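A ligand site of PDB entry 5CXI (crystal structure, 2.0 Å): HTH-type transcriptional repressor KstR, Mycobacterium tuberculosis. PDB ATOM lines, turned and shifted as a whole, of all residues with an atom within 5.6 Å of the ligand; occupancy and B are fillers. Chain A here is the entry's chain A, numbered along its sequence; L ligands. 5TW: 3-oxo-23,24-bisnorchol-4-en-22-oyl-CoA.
NH2 of Arg 162 sits close to OG of Ser 165 (3.3 Å). The side-chain carboxylate (OE1) of Glu 137 is in salt-bridge range of the guanidinium group (NH1) of Arg 162 (3.5 Å). The backbone carbonyl oxygen (O) of Ala 107 sits at hydrogen-bond distance from the side-chain amide nitrogen (ND2) of Asn 111 (2.9 Å). OG of Ser 165 sits at hydrogen-bond distance from OD1 of Asp 141 (3.1 Å). The side-chain hydroxyl of Thr 115 is in hydrogen-bond range of the backbone carbonyl oxygen of Met 108 (3.4 Å). The backbone carbonyl oxygen of Asn 111 sits at hydrogen-bond distance from the side-chain hydroxyl of Thr 115 (2.8 Å). The backbone carbonyl oxygen (O) of Thr 115 lies within hydrogen-bond range of the side-chain hydroxyl (OG1) of Thr 119, at 2.5 Å. NE1 of Trp 168 sits at hydrogen-bond distance from SD of Met 108.
The side-chain carboxylate (OE1) of Glu 75 lies within hydrogen-bond range of a nitrogen (N34) of the ligand, at 2.6 Å. The guanidinium group (NH2) of Arg 162 lies within hydrogen-bond range of an oxygen (O22) of the ligand (3.1 Å). N of Met 108 sits close to S01 of the ligand.
The backbone carbonyl oxygen of Ala 107 sits close to a sulfur (S01) of the ligand (3.3 Å). CD1 of Leu 72 touches C15 of the ligand (3.9 Å). CZ of Phe 76 touches C17 of the ligand, at 3.5 Å. Ile 79 touches the ligand. Asn 111 touches the ligand. Leu 114 touches the ligand (CD2 to O06, 3.5 Å). Thr 115 touches the ligand. Met 118 touches the ligand (CG to C03, 3.6 Å). CZ of Tyr 122 touches C08 of the ligand, at 3.4 Å. Ile 140 touches the ligand (CG2 to O22, 3.9 Å). Ser 165 touches the ligand (OG to C10, 3.5 Å). Trp 168 touches the ligand. Leu 169 touches the ligand. CD1 of Leu 172 touches C21 of the ligand (3.8 Å). Hydrophobic or aromatic side chains that line the ligand: Leu 72, Phe 76, Ile 79, Ala 107, Leu 114, Met 118, Tyr 122, Ile 140, Trp 168 and Leu 172. Within 4 Å of the ligand: Leu 72, Glu 75, Phe 76, Ile 79, Ala 107, Met 108, Asn 111, Leu 114, Thr 115, Met 118, Tyr 122, Ile 140, Arg 162, Ser 165, Trp 168, Leu 169 and Leu 172.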
ATOM      1  N   MET A  30      14.129 -24.849  -0.203  1.00  0.00           N
ATOM      2  CA  MET A  30      13.202 -25.603  -1.036  1.00  0.00           C
ATOM      3  C   MET A  30      11.905 -25.930  -0.295  1.00  0.00           C
ATOM      4  O   MET A  30      10.815 -25.808  -0.860  1.00  0.00           O
ATOM      5  CB  MET A  30      13.864 -26.891  -1.530  1.00  0.00           C
ATOM      6  CG  MET A  30      15.033 -26.655  -2.480  1.00  0.00           C
ATOM      7  SD  MET A  30      14.495 -26.020  -4.082  1.00  0.00           S
ATOM      8  CE  MET A  30      13.792 -27.499  -4.797  1.00  0.00           C
ATOM      9  N   LEU A  72      17.749 -23.871  -6.963  1.00  0.00           N
ATOM     10  CA  LEU A  72      17.322 -24.320  -8.284  1.00  0.00           C
ATOM     11  C   LEU A  72      18.463 -25.041  -8.970  1.00  0.00           C
ATOM     12  O   LEU A  72      18.280 -26.121  -9.539  1.00  0.00           O
ATOM     13  CB  LEU A  72      16.851 -23.137  -9.131  1.00  0.00           C
ATOM     14  CG  LEU A  72      16.231 -23.518 -10.478  1.00  0.00           C
ATOM     15  CD1 LEU A  72      15.031 -24.432 -10.273  1.00  0.00           C
ATOM     16  CD2 LEU A  72      15.840 -22.264 -11.256  1.00  0.00           C
ATOM     17  N   GLU A  75      18.911 -28.395  -7.578  1.00  0.00           N
ATOM     18  CA  GLU A  75      17.824 -29.253  -8.035  1.00  0.00           C
ATOM     19  C   GLU A  75      18.099 -29.780  -9.446  1.00  0.00           C
ATOM     20  O   GLU A  75      17.877 -30.955  -9.736  1.00  0.00           O
ATOM     21  CB  GLU A  75      16.497 -28.504  -7.988  1.00  0.00           C
ATOM     22  CG  GLU A  75      15.275 -29.380  -8.220  1.00  0.00           C
ATOM     23  CD  GLU A  75      14.924 -30.245  -7.012  1.00  0.00           C
ATOM     24  OE1 GLU A  75      13.985 -31.061  -7.123  1.00  0.00           O
ATOM     25  OE2 GLU A  75      15.584 -30.104  -5.967  1.00  0.00           O
ATOM     26  N   PHE A  76      18.565 -28.899 -10.320  1.00  0.00           N
ATOM     27  CA  PHE A  76      18.927 -29.290 -11.680  1.00  0.00           C
ATOM     28  C   PHE A  76      20.092 -30.276 -11.674  1.00  0.00           C
ATOM     29  O   PHE A  76      20.072 -31.272 -12.387  1.00  0.00           O
ATOM     30  CB  PHE A  76      19.295 -28.057 -12.516  1.00  0.00           C
ATOM     31  CG  PHE A  76      18.116 -27.221 -12.902  1.00  0.00           C
ATOM     32  CD1 PHE A  76      16.837 -27.734 -12.870  1.00  0.00           C
ATOM     33  CD2 PHE A  76      18.299 -25.911 -13.314  1.00  0.00           C
ATOM     34  CE1 PHE A  76      15.753 -26.957 -13.232  1.00  0.00           C
ATOM     35  CE2 PHE A  76      17.214 -25.134 -13.675  1.00  0.00           C
ATOM     36  CZ  PHE A  76      15.945 -25.656 -13.632  1.00  0.00           C
ATOM     37  N   ILE A  79      18.702 -33.542 -10.771  1.00  0.00           N
ATOM     38  CA  ILE A  79      17.884 -34.108 -11.833  1.00  0.00           C
ATOM     39  C   ILE A  79      18.781 -34.717 -12.911  1.00  0.00           C
ATOM     40  O   ILE A  79      18.456 -35.752 -13.494  1.00  0.00           O
ATOM     41  CB  ILE A  79      16.928 -33.057 -12.415  1.00  0.00           C
ATOM     42  CG1 ILE A  79      15.821 -32.729 -11.410  1.00  0.00           C
ATOM     43  CG2 ILE A  79      16.329 -33.522 -13.740  1.00  0.00           C
ATOM     44  CD1 ILE A  79      14.826 -31.690 -11.910  1.00  0.00           C
ATOM     45  N   LEU A 104      10.858 -32.078 -17.259  1.00  0.00           N
ATOM     46  CA  LEU A 104      10.914 -30.822 -16.513  1.00  0.00           C
ATOM     47  C   LEU A 104       9.554 -30.119 -16.485  1.00  0.00           C
ATOM     48  O   LEU A 104       9.222 -29.411 -15.528  1.00  0.00           O
ATOM     49  CB  LEU A 104      11.982 -29.900 -17.107  1.00  0.00           C
ATOM     50  CG  LEU A 104      13.418 -30.288 -16.747  1.00  0.00           C
ATOM     51  CD1 LEU A 104      14.419 -29.571 -17.626  1.00  0.00           C
ATOM     52  CD2 LEU A 104      13.686 -30.002 -15.276  1.00  0.00           C
ATOM     53  N   ALA A 107       7.333 -31.831 -13.997  1.00  0.00           N
ATOM     54  CA  ALA A 107       7.902 -31.406 -12.721  1.00  0.00           C
ATOM     55  C   ALA A 107       7.380 -30.016 -12.340  1.00  0.00           C
ATOM     56  O   ALA A 107       7.006 -29.772 -11.188  1.00  0.00           O
ATOM     57  CB  ALA A 107       9.418 -31.405 -12.776  1.00  0.00           C
ATOM     58  N   MET A 108       7.331 -29.121 -13.316  1.00  0.00           N
ATOM     59  CA  MET A 108       6.803 -27.780 -13.114  1.00  0.00           C
ATOM     60  C   MET A 108       5.327 -27.813 -12.727  1.00  0.00           C
ATOM     61  O   MET A 108       4.900 -27.136 -11.795  1.00  0.00           O
ATOM     62  CB  MET A 108       6.984 -26.934 -14.372  1.00  0.00           C
ATOM     63  CG  MET A 108       6.433 -25.525 -14.289  1.00  0.00           C
ATOM     64  SD  MET A 108       6.432 -24.683 -15.880  1.00  0.00           S
ATOM     65  CE  MET A 108       5.154 -25.592 -16.748  1.00  0.00           C
ATOM     66  N   ASN A 111       4.498 -28.745  -9.104  1.00  0.00           N
ATOM     67  CA  ASN A 111       4.916 -27.821  -8.050  1.00  0.00           C
ATOM     68  C   ASN A 111       4.710 -26.359  -8.429  1.00  0.00           C
ATOM     69  O   ASN A 111       5.674 -25.663  -8.750  1.00  0.00           O
ATOM     70  CB  ASN A 111       6.391 -28.053  -7.697  1.00  0.00           C
ATOM     71  CG  ASN A 111       6.684 -29.490  -7.343  1.00  0.00           C
ATOM     72  OD1 ASN A 111       6.555 -29.894  -6.194  1.00  0.00           O
ATOM     73  ND2 ASN A 111       7.095 -30.275  -8.345  1.00  0.00           N
ATOM     74  N   LEU A 114       6.554 -23.695  -5.841  1.00  0.00           N
ATOM     75  CA  LEU A 114       7.991 -23.676  -6.078  1.00  0.00           C
ATOM     76  C   LEU A 114       8.317 -22.932  -7.375  1.00  0.00           C
ATOM     77  O   LEU A 114       9.250 -22.134  -7.420  1.00  0.00           O
ATOM     78  CB  LEU A 114       8.552 -25.106  -6.141  1.00  0.00           C
ATOM     79  CG  LEU A 114      10.062 -25.214  -6.353  1.00  0.00           C
ATOM     80  CD1 LEU A 114      10.815 -24.747  -5.115  1.00  0.00           C
ATOM     81  CD2 LEU A 114      10.459 -26.634  -6.725  1.00  0.00           C
ATOM     82  N   THR A 115       7.520 -23.199  -8.407  1.00  0.00           N
ATOM     83  CA  THR A 115       7.686 -22.546  -9.698  1.00  0.00           C
ATOM     84  C   THR A 115       7.482 -21.042  -9.571  1.00  0.00           C
ATOM     85  O   THR A 115       8.193 -20.255 -10.205  1.00  0.00           O
ATOM     86  CB  THR A 115       6.704 -23.117 -10.744  1.00  0.00           C
ATOM     87  OG1 THR A 115       6.964 -24.512 -10.944  1.00  0.00           O
ATOM     88  CG2 THR A 115       6.864 -22.391 -12.078  1.00  0.00           C
ATOM     89  N   MET A 118      10.636 -19.595  -7.781  1.00  0.00           N
ATOM     90  CA  MET A 118      11.772 -19.576  -8.689  1.00  0.00           C
ATOM     91  C   MET A 118      11.630 -18.523  -9.788  1.00  0.00           C
ATOM     92  O   MET A 118      12.583 -17.813 -10.098  1.00  0.00           O
ATOM     93  CB  MET A 118      11.966 -20.956  -9.318  1.00  0.00           C
ATOM     94  CG  MET A 118      12.337 -22.037  -8.312  1.00  0.00           C
ATOM     95  SD  MET A 118      13.847 -21.629  -7.419  1.00  0.00           S
ATOM     96  CE  MET A 118      13.995 -23.067  -6.362  1.00  0.00           C
ATOM     97  N   THR A 119      10.438 -18.447 -10.376  1.00  0.00           N
ATOM     98  CA  THR A 119      10.184 -17.490 -11.441  1.00  0.00           C
ATOM     99  C   THR A 119      10.354 -16.068 -10.918  1.00  0.00           C
ATOM    100  O   THR A 119      10.988 -15.226 -11.561  1.00  0.00           O
ATOM    101  CB  THR A 119       8.777 -17.655 -12.032  1.00  0.00           C
ATOM    102  OG1 THR A 119       8.556 -19.025 -12.361  1.00  0.00           O
ATOM    103  CG2 THR A 119       8.621 -16.805 -13.292  1.00  0.00           C
ATOM    104  N   TYR A 122      13.971 -15.285 -10.451  1.00  0.00           N
ATOM    105  CA  TYR A 122      14.603 -14.961 -11.721  1.00  0.00           C
ATOM    106  C   TYR A 122      14.247 -13.540 -12.150  1.00  0.00           C
ATOM    107  O   TYR A 122      15.086 -12.830 -12.696  1.00  0.00           O
ATOM    108  CB  TYR A 122      14.182 -15.960 -12.805  1.00  0.00           C
ATOM    109  CG  TYR A 122      15.346 -16.669 -13.432  1.00  0.00           C
ATOM    110  CD1 TYR A 122      15.955 -16.175 -14.580  1.00  0.00           C
ATOM    111  CD2 TYR A 122      15.863 -17.832 -12.867  1.00  0.00           C
ATOM    112  CE1 TYR A 122      17.031 -16.826 -15.151  1.00  0.00           C
ATOM    113  CE2 TYR A 122      16.944 -18.492 -13.440  1.00  0.00           C
ATOM    114  CZ  TYR A 122      17.519 -17.981 -14.582  1.00  0.00           C
ATOM    115  OH  TYR A 122      18.590 -18.623 -15.152  1.00  0.00           O
ATOM    116  N   VAL A 136      22.891 -21.655 -13.057  1.00  0.00           N
ATOM    117  CA  VAL A 136      21.631 -22.243 -13.478  1.00  0.00           C
ATOM    118  C   VAL A 136      21.627 -22.345 -14.995  1.00  0.00           C
ATOM    119  O   VAL A 136      21.395 -23.427 -15.561  1.00  0.00           O
ATOM    120  CB  VAL A 136      20.434 -21.428 -12.960  1.00  0.00           C
ATOM    121  CG1 VAL A 136      19.194 -21.739 -13.780  1.00  0.00           C
ATOM    122  CG2 VAL A 136      20.180 -21.741 -11.483  1.00  0.00           C
ATOM    123  N   GLU A 137      21.916 -21.227 -15.666  1.00  0.00           N
ATOM    124  CA  GLU A 137      21.831 -21.176 -17.121  1.00  0.00           C
ATOM    125  C   GLU A 137      22.749 -22.194 -17.778  1.00  0.00           C
ATOM    126  O   GLU A 137      22.358 -22.890 -18.714  1.00  0.00           O
ATOM    127  CB  GLU A 137      22.155 -19.777 -17.639  1.00  0.00           C
ATOM    128  CG  GLU A 137      21.072 -18.747 -17.358  1.00  0.00           C
ATOM    129  CD  GLU A 137      21.212 -17.508 -18.222  1.00  0.00           C
ATOM    130  OE1 GLU A 137      22.131 -17.463 -19.057  1.00  0.00           O
ATOM    131  OE2 GLU A 137      20.388 -16.577 -18.062  1.00  0.00           O
ATOM    132  N   ILE A 140      21.076 -25.924 -17.012  1.00  0.00           N
ATOM    133  CA  ILE A 140      19.859 -26.263 -17.743  1.00  0.00           C
ATOM    134  C   ILE A 140      20.148 -26.404 -19.241  1.00  0.00           C
ATOM    135  O   ILE A 140      19.800 -27.412 -19.846  1.00  0.00           O
ATOM    136  CB  ILE A 140      18.733 -25.235 -17.446  1.00  0.00           C
ATOM    137  CG1 ILE A 140      17.434 -25.629 -18.161  1.00  0.00           C
ATOM    138  CG2 ILE A 140      19.157 -23.808 -17.789  1.00  0.00           C
ATOM    139  N   ASP A 141      20.838 -25.423 -19.821  1.00  0.00           N
ATOM    140  CA  ASP A 141      21.224 -25.477 -21.227  1.00  0.00           C
ATOM    141  C   ASP A 141      21.993 -26.752 -21.504  1.00  0.00           C
ATOM    142  O   ASP A 141      21.698 -27.462 -22.475  1.00  0.00           O
ATOM    143  CB  ASP A 141      22.050 -24.258 -21.631  1.00  0.00           C
ATOM    144  CG  ASP A 141      21.234 -22.987 -21.691  1.00  0.00           C
ATOM    145  OD1 ASP A 141      19.988 -23.079 -21.647  1.00  0.00           O
ATOM    146  OD2 ASP A 141      21.839 -21.897 -21.808  1.00  0.00           O
ATOM    147  N   PHE A 144      19.799 -29.610 -21.755  1.00  0.00           N
ATOM    148  CA  PHE A 144      19.076 -29.674 -23.010  1.00  0.00           C
ATOM    149  C   PHE A 144      20.045 -30.144 -24.100  1.00  0.00           C
ATOM    150  O   PHE A 144      19.713 -31.043 -24.884  1.00  0.00           O
ATOM    151  CB  PHE A 144      18.471 -28.322 -23.368  1.00  0.00           C
ATOM    152  CG  PHE A 144      17.336 -27.898 -22.474  1.00  0.00           C
ATOM    153  CD1 PHE A 144      16.478 -28.831 -21.929  1.00  0.00           C
ATOM    154  CD2 PHE A 144      17.124 -26.550 -22.194  1.00  0.00           C
ATOM    155  CE1 PHE A 144      15.430 -28.441 -21.104  1.00  0.00           C
ATOM    156  CE2 PHE A 144      16.079 -26.157 -21.378  1.00  0.00           C
ATOM    157  CZ  PHE A 144      15.234 -27.096 -20.831  1.00  0.00           C
ATOM    158  N   ARG A 162      19.405 -22.580 -25.225  1.00  0.00           N
ATOM    159  CA  ARG A 162      19.159 -21.236 -24.721  1.00  0.00           C
ATOM    160  C   ARG A 162      17.824 -20.669 -25.224  1.00  0.00           C
ATOM    161  O   ARG A 162      17.096 -20.017 -24.473  1.00  0.00           O
ATOM    162  CB  ARG A 162      20.301 -20.293 -25.108  1.00  0.00           C
ATOM    163  CG  ARG A 162      20.247 -18.935 -24.412  1.00  0.00           C
ATOM    164  CD  ARG A 162      21.049 -18.932 -23.104  1.00  0.00           C
ATOM    165  NE  ARG A 162      20.560 -19.910 -22.139  1.00  0.00           N
ATOM    166  CZ  ARG A 162      19.746 -19.631 -21.131  1.00  0.00           C
ATOM    167  NH1 ARG A 162      19.307 -18.388 -20.955  1.00  0.00           N
ATOM    168  NH2 ARG A 162      19.363 -20.598 -20.303  1.00  0.00           N
ATOM    169  N   SER A 165      15.052 -22.302 -23.224  1.00  0.00           N
ATOM    170  CA  SER A 165      15.042 -21.684 -21.904  1.00  0.00           C
ATOM    171  C   SER A 165      14.379 -20.298 -21.931  1.00  0.00           C
ATOM    172  O   SER A 165      13.654 -19.927 -21.001  1.00  0.00           O
ATOM    173  CB  SER A 165      16.469 -21.568 -21.359  1.00  0.00           C
ATOM    174  OG  SER A 165      17.002 -22.843 -21.057  1.00  0.00           O
ATOM    175  N   TRP A 168      10.618 -20.700 -22.275  1.00  0.00           N
ATOM    176  CA  TRP A 168      10.163 -21.160 -20.966  1.00  0.00           C
ATOM    177  C   TRP A 168       9.982 -19.981 -20.011  1.00  0.00           C
ATOM    178  O   TRP A 168       8.919 -19.801 -19.431  1.00  0.00           O
ATOM    179  CB  TRP A 168      11.137 -22.168 -20.383  1.00  0.00           C
ATOM    180  CG  TRP A 168      10.493 -23.175 -19.488  1.00  0.00           C
ATOM    181  CD1 TRP A 168       9.619 -22.925 -18.480  1.00  0.00           C
ATOM    182  CD2 TRP A 168      10.704 -24.593 -19.511  1.00  0.00           C
ATOM    183  NE1 TRP A 168       9.250 -24.114 -17.877  1.00  0.00           N
ATOM    184  CE2 TRP A 168       9.902 -25.147 -18.495  1.00  0.00           C
ATOM    185  CE3 TRP A 168      11.484 -25.451 -20.297  1.00  0.00           C
ATOM    186  CZ2 TRP A 168       9.854 -26.518 -18.247  1.00  0.00           C
ATOM    187  CZ3 TRP A 168      11.432 -26.813 -20.047  1.00  0.00           C
ATOM    188  CH2 TRP A 168      10.628 -27.334 -19.030  1.00  0.00           C
ATOM    189  N   LEU A 169      11.043 -19.191 -19.862  1.00  0.00           N
ATOM    190  CA  LEU A 169      11.040 -18.080 -18.921  1.00  0.00           C
ATOM    191  C   LEU A 169      10.019 -17.029 -19.313  1.00  0.00           C
ATOM    192  O   LEU A 169       9.275 -16.526 -18.467  1.00  0.00           O
ATOM    193  CB  LEU A 169      12.425 -17.451 -18.811  1.00  0.00           C
ATOM    194  CG  LEU A 169      12.475 -16.154 -17.996  1.00  0.00           C
ATOM    195  CD1 LEU A 169      12.019 -16.411 -16.565  1.00  0.00           C
ATOM    196  CD2 LEU A 169      13.865 -15.543 -18.016  1.00  0.00           C
ATOM    197  N   LEU A 172       6.620 -18.241 -18.543  1.00  0.00           N
ATOM    198  CA  LEU A 172       6.458 -18.266 -17.092  1.00  0.00           C
ATOM    199  C   LEU A 172       6.203 -16.862 -16.569  1.00  0.00           C
ATOM    200  O   LEU A 172       5.568 -16.694 -15.523  1.00  0.00           O
ATOM    201  CB  LEU A 172       7.691 -18.849 -16.408  1.00  0.00           C
ATOM    202  CG  LEU A 172       7.816 -20.378 -16.370  1.00  0.00           C
ATOM    203  CD1 LEU A 172       8.989 -20.789 -15.496  1.00  0.00           C
ATOM    204  CD2 LEU A 172       6.525 -21.009 -15.865  1.00  0.00           C
HETATM  205  C10 5TW L   1      15.663 -22.001 -17.925  1.00  0.00           C
HETATM  206  C19 5TW L   1      11.692 -26.882 -13.409  1.00  0.00           C
HETATM  207  C11 5TW L   1      14.458 -22.463 -17.369  1.00  0.00           C
HETATM  208  C12 5TW L   1      13.958 -23.679 -17.872  1.00  0.00           C
HETATM  209  C13 5TW L   1      13.845 -21.834 -16.254  1.00  0.00           C
HETATM  210  C18 5TW L   1      11.906 -26.336 -14.847  1.00  0.00           C
HETATM  211  C17 5TW L   1      12.650 -25.055 -14.533  1.00  0.00           C
HETATM  212  C20 5TW L   1      10.376 -24.190 -13.920  1.00  0.00           C
HETATM  213  C21 5TW L   1      12.575 -21.147 -16.743  1.00  0.00           C
HETATM  214  C16 5TW L   1      11.805 -24.492 -13.429  1.00  0.00           C
HETATM  215  C15 5TW L   1      12.481 -23.228 -12.908  1.00  0.00           C
HETATM  216  C14 5TW L   1      12.662 -22.233 -14.053  1.00  0.00           C
HETATM  217  S01 5TW L   1       9.898 -28.289 -10.643  1.00  0.00           S
HETATM  218  C02 5TW L   1      11.049 -26.984 -10.526  1.00  0.00           C
HETATM  219  C03 5TW L   1      10.768 -24.534 -10.458  1.00  0.00           C
HETATM  220  C04 5TW L   1      10.768 -25.751 -11.383  1.00  0.00           C
HETATM  221  C05 5TW L   1      11.857 -25.676 -12.471  1.00  0.00           C
HETATM  222  O06 5TW L   1      12.056 -27.028  -9.816  1.00  0.00           O
HETATM  223  C07 5TW L   1      14.738 -20.790 -15.551  1.00  0.00           C
HETATM  224  C08 5TW L   1      15.542 -19.964 -16.566  1.00  0.00           C
HETATM  225  C09 5TW L   1      16.190 -20.777 -17.522  1.00  0.00           C
HETATM  226  O22 5TW L   1      17.243 -20.400 -18.020  1.00  0.00           O
HETATM  227  C23 5TW L   1      13.514 -22.870 -15.159  1.00  0.00           C
HETATM  228  C24 5TW L   1      12.791 -24.089 -15.692  1.00  0.00           C
HETATM  229  C25 5TW L   1      13.664 -24.699 -16.769  1.00  0.00           C
HETATM  230  C32 5TW L   1      11.799 -30.266 -10.115  1.00  0.00           C
HETATM  231  C33 5TW L   1      10.651 -29.480  -9.486  1.00  0.00           C
HETATM  232  N34 5TW L   1      12.322 -31.243  -9.136  1.00  0.00           N
HETATM  233  C35 5TW L   1      11.891 -32.512  -9.054  1.00  0.00           C
HETATM  234  O36 5TW L   1      11.020 -32.976  -9.779  1.00  0.00           O
